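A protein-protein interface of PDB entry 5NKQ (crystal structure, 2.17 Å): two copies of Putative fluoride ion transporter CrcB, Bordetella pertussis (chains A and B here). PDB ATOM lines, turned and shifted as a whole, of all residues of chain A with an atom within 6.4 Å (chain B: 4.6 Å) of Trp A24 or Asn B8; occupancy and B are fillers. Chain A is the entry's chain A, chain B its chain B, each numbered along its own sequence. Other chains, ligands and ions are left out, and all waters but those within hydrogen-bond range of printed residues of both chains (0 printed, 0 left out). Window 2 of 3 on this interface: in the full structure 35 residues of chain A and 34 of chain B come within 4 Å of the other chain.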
ATOM      1  N   GLY A  19     -23.802  26.943  36.510  1.00  0.00           N
ATOM      2  CA  GLY A  19     -22.784  27.300  35.536  1.00  0.00           C
ATOM      3  C   GLY A  19     -22.995  26.625  34.194  1.00  0.00           C
ATOM      4  O   GLY A  19     -22.782  27.237  33.143  1.00  0.00           O
ATOM      5  N   ALA A  20     -23.415  25.358  34.208  1.00  0.00           N
ATOM      6  CA  ALA A  20     -23.685  24.658  32.958  1.00  0.00           C
ATOM      7  C   ALA A  20     -24.939  25.190  32.279  1.00  0.00           C
ATOM      8  O   ALA A  20     -25.009  25.219  31.044  1.00  0.00           O
ATOM      9  CB  ALA A  20     -23.814  23.158  33.212  1.00  0.00           C
ATOM     10  N   TRP A  21     -25.938  25.606  33.061  1.00  0.00           N
ATOM     11  CA  TRP A  21     -27.122  26.228  32.477  1.00  0.00           C
ATOM     12  C   TRP A  21     -26.766  27.535  31.781  1.00  0.00           C
ATOM     13  O   TRP A  21     -27.290  27.837  30.703  1.00  0.00           O
ATOM     14  CB  TRP A  21     -28.178  26.470  33.558  1.00  0.00           C
ATOM     15  CG  TRP A  21     -28.896  25.232  34.002  1.00  0.00           C
ATOM     16  CD1 TRP A  21     -28.818  23.991  33.441  1.00  0.00           C
ATOM     17  CD2 TRP A  21     -29.806  25.118  35.102  1.00  0.00           C
ATOM     18  NE1 TRP A  21     -29.623  23.110  34.124  1.00  0.00           N
ATOM     19  CE2 TRP A  21     -30.241  23.778  35.149  1.00  0.00           C
ATOM     20  CE3 TRP A  21     -30.296  26.020  36.053  1.00  0.00           C
ATOM     21  CZ2 TRP A  21     -31.143  23.318  36.108  1.00  0.00           C
ATOM     22  CZ3 TRP A  21     -31.190  25.561  37.006  1.00  0.00           C
ATOM     23  CH2 TRP A  21     -31.603  24.223  37.026  1.00  0.00           C
ATOM     24  N   LEU A  22     -25.872  28.323  32.384  1.00  0.00           N
ATOM     25  CA  LEU A  22     -25.479  29.593  31.783  1.00  0.00           C
ATOM     26  C   LEU A  22     -24.686  29.377  30.501  1.00  0.00           C
ATOM     27  O   LEU A  22     -24.917  30.065  29.499  1.00  0.00           O
ATOM     28  CB  LEU A  22     -24.672  30.419  32.785  1.00  0.00           C
ATOM     29  CG  LEU A  22     -24.149  31.763  32.278  1.00  0.00           C
ATOM     30  CD1 LEU A  22     -25.291  32.613  31.739  1.00  0.00           C
ATOM     31  CD2 LEU A  22     -23.403  32.496  33.382  1.00  0.00           C
ATOM     32  N   ARG A  23     -23.743  28.431  30.511  1.00  0.00           N
ATOM     33  CA  ARG A  23     -22.990  28.129  29.298  1.00  0.00           C
ATOM     34  C   ARG A  23     -23.907  27.613  28.196  1.00  0.00           C
ATOM     35  O   ARG A  23     -23.739  27.962  27.022  1.00  0.00           O
ATOM     36  CB  ARG A  23     -21.889  27.113  29.603  1.00  0.00           C
ATOM     37  CG  ARG A  23     -21.295  26.449  28.371  1.00  0.00           C
ATOM     38  CD  ARG A  23     -20.085  25.601  28.726  1.00  0.00           C
ATOM     39  NE  ARG A  23     -20.327  24.751  29.887  1.00  0.00           N
ATOM     40  CZ  ARG A  23     -20.823  23.520  29.824  1.00  0.00           C
ATOM     41  NH1 ARG A  23     -21.133  22.989  28.649  1.00  0.00           N
ATOM     42  NH2 ARG A  23     -21.010  22.820  30.934  1.00  0.00           N
ATOM     43  N   TRP A  24     -24.892  26.788  28.561  1.00  0.00           N
ATOM     44  CA  TRP A  24     -25.831  26.267  27.574  1.00  0.00           C
ATOM     45  C   TRP A  24     -26.650  27.389  26.944  1.00  0.00           C
ATOM     46  O   TRP A  24     -26.843  27.415  25.723  1.00  0.00           O
ATOM     47  CB  TRP A  24     -26.741  25.229  28.230  1.00  0.00           C
ATOM     48  CG  TRP A  24     -27.803  24.680  27.331  1.00  0.00           C
ATOM     49  CD1 TRP A  24     -27.628  24.114  26.101  1.00  0.00           C
ATOM     50  CD2 TRP A  24     -29.209  24.621  27.602  1.00  0.00           C
ATOM     51  NE1 TRP A  24     -28.837  23.717  25.586  1.00  0.00           N
ATOM     52  CE2 TRP A  24     -29.824  24.016  26.488  1.00  0.00           C
ATOM     53  CE3 TRP A  24     -30.006  25.024  28.677  1.00  0.00           C
ATOM     54  CZ2 TRP A  24     -31.199  23.807  26.418  1.00  0.00           C
ATOM     55  CZ3 TRP A  24     -31.371  24.816  28.606  1.00  0.00           C
ATOM     56  CH2 TRP A  24     -31.954  24.212  27.484  1.00  0.00           C
ATOM     57  N   VAL A  25     -27.128  28.330  27.760  1.00  0.00           N
ATOM     58  CA  VAL A  25     -27.905  29.447  27.229  1.00  0.00           C
ATOM     59  C   VAL A  25     -27.025  30.355  26.379  1.00  0.00           C
ATOM     60  O   VAL A  25     -27.431  30.800  25.297  1.00  0.00           O
ATOM     61  CB  VAL A  25     -28.581  30.219  28.376  1.00  0.00           C
ATOM     62  CG1 VAL A  25     -29.188  31.515  27.862  1.00  0.00           C
ATOM     63  CG2 VAL A  25     -29.648  29.359  29.036  1.00  0.00           C
ATOM     64  N   LEU A  26     -25.807  30.645  26.850  1.00  0.00           N
ATOM     65  CA  LEU A  26     -24.894  31.482  26.076  1.00  0.00           C
ATOM     66  C   LEU A  26     -24.603  30.870  24.713  1.00  0.00           C
ATOM     67  O   LEU A  26     -24.495  31.587  23.712  1.00  0.00           O
ATOM     68  CB  LEU A  26     -23.595  31.702  26.852  1.00  0.00           C
ATOM     69  CG  LEU A  26     -23.639  32.699  28.011  1.00  0.00           C
ATOM     70  CD1 LEU A  26     -22.355  32.634  28.822  1.00  0.00           C
ATOM     71  CD2 LEU A  26     -23.872  34.109  27.489  1.00  0.00           C
ATOM     72  N   GLY A  27     -24.477  29.543  24.653  1.00  0.00           N
ATOM     73  CA  GLY A  27     -24.252  28.892  23.374  1.00  0.00           C
ATOM     74  C   GLY A  27     -25.446  29.001  22.446  1.00  0.00           C
ATOM     75  O   GLY A  27     -25.290  29.232  21.245  1.00  0.00           O
ATOM     76  N   LEU A  28     -26.655  28.842  22.988  1.00  0.00           N
ATOM     77  CA  LEU A  28     -27.849  28.938  22.157  1.00  0.00           C
ATOM     78  C   LEU A  28     -28.045  30.347  21.608  1.00  0.00           C
ATOM     79  O   LEU A  28     -28.627  30.513  20.530  1.00  0.00           O
ATOM     80  CB  LEU A  28     -29.081  28.505  22.954  1.00  0.00           C
ATOM     81  CG  LEU A  28     -29.103  27.052  23.432  1.00  0.00           C
ATOM     82  CD1 LEU A  28     -30.348  26.778  24.263  1.00  0.00           C
ATOM     83  CD2 LEU A  28     -29.022  26.097  22.251  1.00  0.00           C
ATOM     84  N   LYS A  29     -27.560  31.365  22.318  1.00  0.00           N
ATOM     85  CA  LYS A  29     -27.772  32.748  21.917  1.00  0.00           C
ATOM     86  C   LYS A  29     -26.581  33.373  21.202  1.00  0.00           C
ATOM     87  O   LYS A  29     -26.767  34.362  20.484  1.00  0.00           O
ATOM     88  CB  LYS A  29     -28.121  33.610  23.137  1.00  0.00           C
ATOM     89  CG  LYS A  29     -29.476  33.299  23.754  1.00  0.00           C
ATOM     90  CD  LYS A  29     -29.786  34.243  24.907  1.00  0.00           C
ATOM     91  CE  LYS A  29     -31.166  33.977  25.486  1.00  0.00           C
ATOM     92  NZ  LYS A  29     -32.238  34.162  24.470  1.00  0.00           N
ATOM     93  N   ALA B   5     -36.826  23.757  27.577  1.00  0.00           N
ATOM     94  CA  ALA B   5     -37.581  22.639  28.130  1.00  0.00           C
ATOM     95  C   ALA B   5     -37.033  22.236  29.495  1.00  0.00           C
ATOM     96  O   ALA B   5     -35.821  22.266  29.713  1.00  0.00           O
ATOM     97  CB  ALA B   5     -37.551  21.454  27.174  1.00  0.00           C
ATOM     98  N   PRO B   6     -37.926  21.863  30.415  1.00  0.00           N
ATOM     99  CA  PRO B   6     -37.461  21.441  31.747  1.00  0.00           C
ATOM    100  C   PRO B   6     -36.615  20.180  31.718  1.00  0.00           C
ATOM    101  O   PRO B   6     -35.708  20.038  32.547  1.00  0.00           O
ATOM    102  CB  PRO B   6     -38.769  21.230  32.523  1.00  0.00           C
ATOM    103  CG  PRO B   6     -39.801  20.984  31.471  1.00  0.00           C
ATOM    104  CD  PRO B   6     -39.393  21.828  30.301  1.00  0.00           C
ATOM    105  N   LEU B   7     -36.882  19.262  30.785  1.00  0.00           N
ATOM    106  CA  LEU B   7     -36.060  18.060  30.673  1.00  0.00           C
ATOM    107  C   LEU B   7     -34.621  18.408  30.316  1.00  0.00           C
ATOM    108  O   LEU B   7     -33.682  17.750  30.777  1.00  0.00           O
ATOM    109  CB  LEU B   7     -36.657  17.113  29.633  1.00  0.00           C
ATOM    110  CG  LEU B   7     -35.846  15.859  29.290  1.00  0.00           C
ATOM    111  CD1 LEU B   7     -35.806  14.895  30.468  1.00  0.00           C
ATOM    112  CD2 LEU B   7     -36.400  15.177  28.048  1.00  0.00           C
ATOM    113  N   ASN B   8     -34.428  19.444  29.496  1.00  0.00           N
ATOM    114  CA  ASN B   8     -33.077  19.850  29.123  1.00  0.00           C
ATOM    115  C   ASN B   8     -32.314  20.401  30.322  1.00  0.00           C
ATOM    116  O   ASN B   8     -31.119  20.129  30.479  1.00  0.00           O
ATOM    117  CB  ASN B   8     -33.128  20.880  27.996  1.00  0.00           C
ATOM    118  CG  ASN B   8     -33.652  20.298  26.699  1.00  0.00           C
ATOM    119  OD1 ASN B   8     -33.546  19.095  26.459  1.00  0.00           O
ATOM    120  ND2 ASN B   8     -34.216  21.150  25.851  1.00  0.00           N
ATOM    121  N   PHE B   9     -32.986  21.180  31.173  1.00  0.00           N
ATOM    122  CA  PHE B   9     -32.337  21.683  32.379  1.00  0.00           C
ATOM    123  C   PHE B   9     -31.974  20.546  33.325  1.00  0.00           C
ATOM    124  O   PHE B   9     -30.932  20.586  33.988  1.00  0.00           O
ATOM    125  CB  PHE B   9     -33.241  22.696  33.085  1.00  0.00           C
ATOM    126  CG  PHE B   9     -33.259  24.054  32.440  1.00  0.00           C
ATOM    127  CD1 PHE B   9     -32.329  25.016  32.798  1.00  0.00           C
ATOM    128  CD2 PHE B   9     -34.210  24.370  31.483  1.00  0.00           C
ATOM    129  CE1 PHE B   9     -32.343  26.268  32.210  1.00  0.00           C
ATOM    130  CE2 PHE B   9     -34.229  25.621  30.892  1.00  0.00           C
ATOM    131  CZ  PHE B   9     -33.294  26.571  31.255  1.00  0.00           C
ATOM    132  N   ILE B  10     -32.822  19.518  33.398  1.00  0.00           N
ATOM    133  CA  ILE B  10     -32.563  18.401  34.300  1.00  0.00           C
ATOM    134  C   ILE B  10     -31.431  17.531  33.768  1.00  0.00           C
ATOM    135  O   ILE B  10     -30.554  17.100  34.527  1.00  0.00           O
ATOM    136  CB  ILE B  10     -33.851  17.587  34.520  1.00  0.00           C
ATOM    137  CG1 ILE B  10     -34.916  18.450  35.198  1.00  0.00           C
ATOM    138  CG2 ILE B  10     -33.564  16.345  35.348  1.00  0.00           C
ATOM    139  CD1 ILE B  10     -36.245  17.752  35.382  1.00  0.00           C
ATOM    140  N   ALA B  11     -31.428  17.262  32.460  1.00  0.00           N
ATOM    141  CA  ALA B  11     -30.378  16.430  31.880  1.00  0.00           C
ATOM    142  C   ALA B  11     -29.015  17.100  31.995  1.00  0.00           C
ATOM    143  O   ALA B  11     -28.012  16.439  32.293  1.00  0.00           O
ATOM    144  CB  ALA B  11     -30.703  16.118  30.419  1.00  0.00           C
ATOM    145  N   ILE B  12     -28.958  18.413  31.765  1.00  0.00           N
ATOM    146  CA  ILE B  12     -27.695  19.134  31.887  1.00  0.00           C
ATOM    147  C   ILE B  12     -27.285  19.251  33.349  1.00  0.00           C
ATOM    148  O   ILE B  12     -26.098  19.146  33.685  1.00  0.00           O
ATOM    149  CB  ILE B  12     -27.809  20.515  31.216  1.00  0.00           C
ATOM    150  CG1 ILE B  12     -28.045  20.354  29.715  1.00  0.00           C
ATOM    151  CG2 ILE B  12     -26.564  21.350  31.476  1.00  0.00           C
ATOM    152  CD1 ILE B  12     -28.371  21.646  29.014  1.00  0.00           C
ATOM    153  N   LEU B  69     -27.261  16.435  25.562  1.00  0.00           N
ATOM    154  CA  LEU B  69     -27.054  17.484  26.552  1.00  0.00           C
ATOM    155  C   LEU B  69     -26.564  16.930  27.884  1.00  0.00           C
ATOM    156  O   LEU B  69     -25.773  17.588  28.570  1.00  0.00           O
ATOM    157  CB  LEU B  69     -28.350  18.272  26.752  1.00  0.00           C
ATOM    158  CG  LEU B  69     -28.887  18.986  25.508  1.00  0.00           C
ATOM    159  CD1 LEU B  69     -30.220  19.662  25.800  1.00  0.00           C
ATOM    160  CD2 LEU B  69     -27.870  19.993  24.993  1.00  0.00           C
ATOM    161  N   THR B  73     -22.853  18.391  26.943  1.00  0.00           N
ATOM    162  CA  THR B  73     -23.068  19.705  27.542  1.00  0.00           C
ATOM    163  C   THR B  73     -23.039  19.627  29.064  1.00  0.00           C
ATOM    164  O   THR B  73     -22.522  20.529  29.732  1.00  0.00           O
ATOM    165  CB  THR B  73     -24.395  20.292  27.059  1.00  0.00           C
ATOM    166  OG1 THR B  73     -24.412  20.326  25.626  1.00  0.00           O
ATOM    167  CG2 THR B  73     -24.583  21.706  27.593  1.00  0.00           C
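The backbone carbonyl oxygen (O) of Thr B73 sits at hydrogen-bond distance from the guanidinium group (NH2) of Arg A23, 3.0 Å away. The indole nitrogen (NE1) of Trp A21 sits at hydrogen-bond distance from the backbone carbonyl oxygen (O) of Phe B9.
Of the printed residues of chain B, Ala A20 touches Ile B12. Printed residues of chain B within 4 Å of Trp A24: Asn B8 (3.6 Å), Phe B9 (3.7 Å), Ile B12 (3.4 Å) and Leu B69 (3.9 Å). Pro B6 touches none of the printed residues of chain A. Of the printed residues of chain A, Asn B8 touches Trp A24. Ala B11 touches none of the printed residues of chain A. Of the printed residues of chain A, Ile B12 touches Ala A20 (3.7 Å), Trp A21 (3.99 Å) and Trp A24 (3.4 Å). The nearest residue of chain B that does not touch Trp A24 is Thr B73 (4.2 Å). The nearest residue of chain A that does not touch Asn B8 is Trp A21 (4.9 Å).
Of the 11 printed residues of chain A, 4 touch a printed residue of chain B.
No position is printed for both chains.
Among the printed residues, merely in contact across the chains: Trp A24 with Ile B12, Trp A24 with Asn B8, Trp A24 with Phe B9, Ala A20 with Ile B12, Trp A24 with Leu B69 and Trp A21 with Ile B12.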
